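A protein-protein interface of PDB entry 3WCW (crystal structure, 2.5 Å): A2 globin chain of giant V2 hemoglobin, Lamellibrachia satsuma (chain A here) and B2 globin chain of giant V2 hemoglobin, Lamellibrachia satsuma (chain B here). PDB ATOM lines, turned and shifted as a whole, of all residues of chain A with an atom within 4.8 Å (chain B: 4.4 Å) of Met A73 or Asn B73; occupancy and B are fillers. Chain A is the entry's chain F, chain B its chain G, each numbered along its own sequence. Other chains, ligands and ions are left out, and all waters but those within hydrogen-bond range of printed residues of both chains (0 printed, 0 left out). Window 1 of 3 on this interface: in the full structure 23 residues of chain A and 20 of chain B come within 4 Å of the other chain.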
ATOM      1  N   GLY A  69      15.928  -6.162  15.890  1.00  0.00           N
ATOM      2  CA  GLY A  69      14.679  -6.603  16.497  1.00  0.00           C
ATOM      3  C   GLY A  69      13.531  -5.639  16.203  1.00  0.00           C
ATOM      4  O   GLY A  69      12.396  -6.052  15.960  1.00  0.00           O
ATOM      5  N   GLY A  70      13.832  -4.340  16.235  1.00  0.00           N
ATOM      6  CA  GLY A  70      12.819  -3.342  15.950  1.00  0.00           C
ATOM      7  C   GLY A  70      12.415  -3.572  14.518  1.00  0.00           C
ATOM      8  O   GLY A  70      11.236  -3.725  14.203  1.00  0.00           O
ATOM      9  N   LEU A  71      13.418  -3.633  13.648  1.00  0.00           N
ATOM     10  CA  LEU A  71      13.179  -3.865  12.226  1.00  0.00           C
ATOM     11  C   LEU A  71      12.318  -5.101  11.983  1.00  0.00           C
ATOM     12  O   LEU A  71      11.431  -5.083  11.141  1.00  0.00           O
ATOM     13  CB  LEU A  71      14.510  -4.013  11.477  1.00  0.00           C
ATOM     14  CG  LEU A  71      14.976  -2.743  10.761  1.00  0.00           C
ATOM     15  CD1 LEU A  71      16.278  -3.011  10.012  1.00  0.00           C
ATOM     16  CD2 LEU A  71      13.892  -2.290   9.786  1.00  0.00           C
ATOM     17  N   ASP A  72      12.586  -6.170  12.726  1.00  0.00           N
ATOM     18  CA  ASP A  72      11.839  -7.408  12.571  1.00  0.00           C
ATOM     19  C   ASP A  72      10.362  -7.184  12.854  1.00  0.00           C
ATOM     20  O   ASP A  72       9.494  -7.628  12.086  1.00  0.00           O
ATOM     21  CB  ASP A  72      12.393  -8.470  13.516  1.00  0.00           C
ATOM     22  CG  ASP A  72      11.804  -9.840  13.260  1.00  0.00           C
ATOM     23  OD1 ASP A  72      10.977 -10.319  14.067  1.00  0.00           O
ATOM     24  OD2 ASP A  72      12.174 -10.436  12.232  1.00  0.00           O
ATOM     25  N   MET A  73      10.080  -6.488  13.955  1.00  0.00           N
ATOM     26  CA  MET A  73       8.702  -6.209  14.339  1.00  0.00           C
ATOM     27  C   MET A  73       7.970  -5.469  13.228  1.00  0.00           C
ATOM     28  O   MET A  73       6.871  -5.856  12.840  1.00  0.00           O
ATOM     29  CB  MET A  73       8.659  -5.395  15.640  1.00  0.00           C
ATOM     30  CG  MET A  73       9.241  -6.131  16.841  1.00  0.00           C
ATOM     31  SD  MET A  73       8.791  -5.412  18.438  1.00  0.00           S
ATOM     32  CE  MET A  73      10.173  -4.284  18.672  1.00  0.00           C
ATOM     33  N   CYS A  74       8.585  -4.416  12.705  1.00  0.00           N
ATOM     34  CA  CYS A  74       7.965  -3.650  11.632  1.00  0.00           C
ATOM     35  C   CYS A  74       7.672  -4.565  10.444  1.00  0.00           C
ATOM     36  O   CYS A  74       6.519  -4.683   9.999  1.00  0.00           O
ATOM     37  CB  CYS A  74       8.877  -2.495  11.190  1.00  0.00           C
ATOM     38  SG  CYS A  74       9.136  -1.228  12.468  1.00  0.00           S
ATOM     39  N   VAL A  75       8.717  -5.219   9.939  1.00  0.00           N
ATOM     40  CA  VAL A  75       8.564  -6.117   8.804  1.00  0.00           C
ATOM     41  C   VAL A  75       7.422  -7.091   9.061  1.00  0.00           C
ATOM     42  O   VAL A  75       6.512  -7.230   8.240  1.00  0.00           O
ATOM     43  CB  VAL A  75       9.873  -6.895   8.541  1.00  0.00           C
ATOM     44  CG1 VAL A  75       9.637  -8.027   7.542  1.00  0.00           C
ATOM     45  CG2 VAL A  75      10.931  -5.930   8.024  1.00  0.00           C
ATOM     46  N   ALA A  76       7.463  -7.749  10.213  1.00  0.00           N
ATOM     47  CA  ALA A  76       6.433  -8.715  10.573  1.00  0.00           C
ATOM     48  C   ALA A  76       5.043  -8.095  10.505  1.00  0.00           C
ATOM     49  O   ALA A  76       4.069  -8.786  10.205  1.00  0.00           O
ATOM     50  CB  ALA A  76       6.695  -9.254  11.976  1.00  0.00           C
ATOM     51  N   LEU A  77       4.962  -6.788  10.770  1.00  0.00           N
ATOM     52  CA  LEU A  77       3.684  -6.082  10.764  1.00  0.00           C
ATOM     53  C   LEU A  77       3.307  -5.337   9.483  1.00  0.00           C
ATOM     54  O   LEU A  77       2.243  -4.730   9.431  1.00  0.00           O
ATOM     55  CB  LEU A  77       3.632  -5.110  11.943  1.00  0.00           C
ATOM     56  CG  LEU A  77       3.715  -5.778  13.315  1.00  0.00           C
ATOM     57  CD1 LEU A  77       3.993  -4.741  14.412  1.00  0.00           C
ATOM     58  CD2 LEU A  77       2.415  -6.522  13.557  1.00  0.00           C
ATOM     59  N   GLN A  87       3.229   0.499  16.374  1.00  0.00           N
ATOM     60  CA  GLN A  87       4.619   0.112  16.587  1.00  0.00           C
ATOM     61  C   GLN A  87       5.600   1.157  16.047  1.00  0.00           C
ATOM     62  O   GLN A  87       6.641   1.419  16.657  1.00  0.00           O
ATOM     63  CB  GLN A  87       4.888  -1.251  15.934  1.00  0.00           C
ATOM     64  CG  GLN A  87       6.284  -1.802  16.187  1.00  0.00           C
ATOM     65  CD  GLN A  87       6.633  -1.808  17.659  1.00  0.00           C
ATOM     66  OE1 GLN A  87       5.802  -2.168  18.497  1.00  0.00           O
ATOM     67  NE2 GLN A  87       7.865  -1.418  17.987  1.00  0.00           N
ATOM     68  N   ILE B  69       3.838  -7.932  20.965  1.00  0.00           N
ATOM     69  CA  ILE B  69       4.907  -8.106  19.992  1.00  0.00           C
ATOM     70  C   ILE B  69       6.200  -7.599  20.597  1.00  0.00           C
ATOM     71  O   ILE B  69       7.253  -8.196  20.398  1.00  0.00           O
ATOM     72  CB  ILE B  69       4.585  -7.356  18.694  1.00  0.00           C
ATOM     73  CG1 ILE B  69       3.483  -8.115  17.952  1.00  0.00           C
ATOM     74  CG2 ILE B  69       5.832  -7.186  17.847  1.00  0.00           C
ATOM     75  CD1 ILE B  69       3.001  -7.415  16.711  1.00  0.00           C
ATOM     76  N   ARG B  70       6.124  -6.505  21.348  1.00  0.00           N
ATOM     77  CA  ARG B  70       7.323  -5.984  21.990  1.00  0.00           C
ATOM     78  C   ARG B  70       7.871  -7.011  22.983  1.00  0.00           C
ATOM     79  O   ARG B  70       9.067  -7.312  22.985  1.00  0.00           O
ATOM     80  CB  ARG B  70       7.030  -4.660  22.708  1.00  0.00           C
ATOM     81  CG  ARG B  70       7.038  -3.442  21.768  1.00  0.00           C
ATOM     82  CD  ARG B  70       7.161  -2.106  22.510  1.00  0.00           C
ATOM     83  NE  ARG B  70       5.949  -1.705  23.227  1.00  0.00           N
ATOM     84  CZ  ARG B  70       4.857  -1.221  22.641  1.00  0.00           C
ATOM     85  NH1 ARG B  70       4.816  -1.076  21.322  1.00  0.00           N
ATOM     86  NH2 ARG B  70       3.801  -0.875  23.375  1.00  0.00           N
ATOM     87  N   VAL B  71       6.991  -7.566  23.809  1.00  0.00           N
ATOM     88  CA  VAL B  71       7.396  -8.553  24.802  1.00  0.00           C
ATOM     89  C   VAL B  71       8.064  -9.753  24.134  1.00  0.00           C
ATOM     90  O   VAL B  71       9.172 -10.157  24.509  1.00  0.00           O
ATOM     91  CB  VAL B  71       6.179  -9.053  25.631  1.00  0.00           C
ATOM     92  CG1 VAL B  71       6.622 -10.103  26.661  1.00  0.00           C
ATOM     93  CG2 VAL B  71       5.515  -7.878  26.335  1.00  0.00           C
ATOM     94  N   VAL B  72       7.386 -10.317  23.143  1.00  0.00           N
ATOM     95  CA  VAL B  72       7.903 -11.470  22.429  1.00  0.00           C
ATOM     96  C   VAL B  72       9.246 -11.188  21.756  1.00  0.00           C
ATOM     97  O   VAL B  72      10.152 -12.019  21.821  1.00  0.00           O
ATOM     98  CB  VAL B  72       6.850 -11.979  21.412  1.00  0.00           C
ATOM     99  CG1 VAL B  72       7.509 -12.716  20.268  1.00  0.00           C
ATOM    100  CG2 VAL B  72       5.894 -12.899  22.126  1.00  0.00           C
ATOM    101  N   ASN B  73       9.386 -10.021  21.126  1.00  0.00           N
ATOM    102  CA  ASN B  73      10.649  -9.658  20.478  1.00  0.00           C
ATOM    103  C   ASN B  73      11.713  -9.647  21.570  1.00  0.00           C
ATOM    104  O   ASN B  73      12.880  -9.976  21.335  1.00  0.00           O
ATOM    105  CB  ASN B  73      10.543  -8.268  19.843  1.00  0.00           C
ATOM    106  CG  ASN B  73      11.838  -7.813  19.209  1.00  0.00           C
ATOM    107  OD1 ASN B  73      12.196  -8.251  18.114  1.00  0.00           O
ATOM    108  ND2 ASN B  73      12.557  -6.934  19.897  1.00  0.00           N
ATOM    109  N   GLY B  74      11.284  -9.277  22.773  1.00  0.00           N
ATOM    110  CA  GLY B  74      12.175  -9.219  23.908  1.00  0.00           C
ATOM    111  C   GLY B  74      12.628 -10.577  24.385  1.00  0.00           C
ATOM    112  O   GLY B  74      13.801 -10.758  24.715  1.00  0.00           O
ATOM    113  N   LEU B  75      11.712 -11.536  24.439  1.00  0.00           N
ATOM    114  CA  LEU B  75      12.077 -12.878  24.889  1.00  0.00           C
ATOM    115  C   LEU B  75      12.949 -13.550  23.824  1.00  0.00           C
ATOM    116  O   LEU B  75      13.905 -14.246  24.153  1.00  0.00           O
ATOM    117  CB  LEU B  75      10.825 -13.724  25.173  1.00  0.00           C
ATOM    118  CG  LEU B  75      11.134 -15.133  25.701  1.00  0.00           C
ATOM    119  CD1 LEU B  75      12.055 -15.034  26.910  1.00  0.00           C
ATOM    120  CD2 LEU B  75       9.851 -15.875  26.053  1.00  0.00           C
ATOM    121  N   ASP B  76      12.622 -13.315  22.552  1.00  0.00           N
ATOM    122  CA  ASP B  76      13.377 -13.870  21.424  1.00  0.00           C
ATOM    123  C   ASP B  76      14.803 -13.322  21.397  1.00  0.00           C
ATOM    124  O   ASP B  76      15.739 -14.042  21.056  1.00  0.00           O
ATOM    125  CB  ASP B  76      12.674 -13.541  20.100  1.00  0.00           C
ATOM    126  CG  ASP B  76      13.416 -14.083  18.887  1.00  0.00           C
ATOM    127  OD1 ASP B  76      14.094 -13.299  18.195  1.00  0.00           O
ATOM    128  OD2 ASP B  76      13.327 -15.300  18.623  1.00  0.00           O
ATOM    129  N   SER B  77      14.980 -12.051  21.748  1.00  0.00           N
ATOM    130  CA  SER B  77      16.323 -11.484  21.748  1.00  0.00           C
ATOM    131  C   SER B  77      17.083 -12.200  22.843  1.00  0.00           C
ATOM    132  O   SER B  77      18.217 -12.630  22.651  1.00  0.00           O
ATOM    133  CB  SER B  77      16.301  -9.983  22.038  1.00  0.00           C
ATOM    134  OG  SER B  77      16.131  -9.736  23.427  1.00  0.00           O
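Of the 9 printed residues of chain B, 3 touch a printed residue of chain A. Printed residues of chain B that touch a printed residue of chain A: Ile B69, Arg B70 and Asn B73. Printed residues of chain A that touch a printed residue of chain B: Gly A69, Met A73, Leu A77 and Gln A87. Hydrophobic or aromatic side chains of chain A within 4 Å of the printed part of chain B: Met A73 and Leu A77. Among the printed residues, 6 pairs touch across the chains. Among the printed residues, no Asp or Glu carboxylate lies within 4 Å of a Lys or Arg side-chain nitrogen of the other chain.
Printed residues of chain B within 4 Å of Gly A69: Asn B73 (3.1 Å). Gly A70 touches none of the printed residues of chain B. Leu A71 touches none of the printed residues of chain B. Of the printed residues of chain B, Met A73 touches Ile B69, Arg B70 and Asn B73. Of the printed residues of chain B, Gln A87 touches Arg B70 (3.2 Å). Of the printed residues of chain A, Ile B69 touches Met A73 and Leu A77. Printed residues of chain A within 4 Å of Arg B70: Met A73 and Gln A87. Of the printed residues of chain A, Asn B73 touches Gly A69 (3.1 Å) and Met A73 (3.6 Å). The nearest printed residue of chain B that does not touch Met A73 is Val B71 (6.1 Å). The nearest printed residue of chain A that does not touch Asn B73 is Asp A72 (4.6 Å).
The side-chain sulfur (SD) of Met A73 lies close to the backbone carbonyl oxygen (O) of Ile B69, at 3.7 Å. OE1 of Gln A87 sits at hydrogen-bond distance from NH1 of Arg B70, 3.2 Å away. OD1 of Asn B73 lies close to O of Gly A69, 3.1 Å away.
Among the printed residues, merely in contact across the chains: Met A73 with Arg B70 (3.9 Å), Met A73 with Asn B73 (3.6 Å) and Leu A77 with Ile B69 (3.3 Å).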
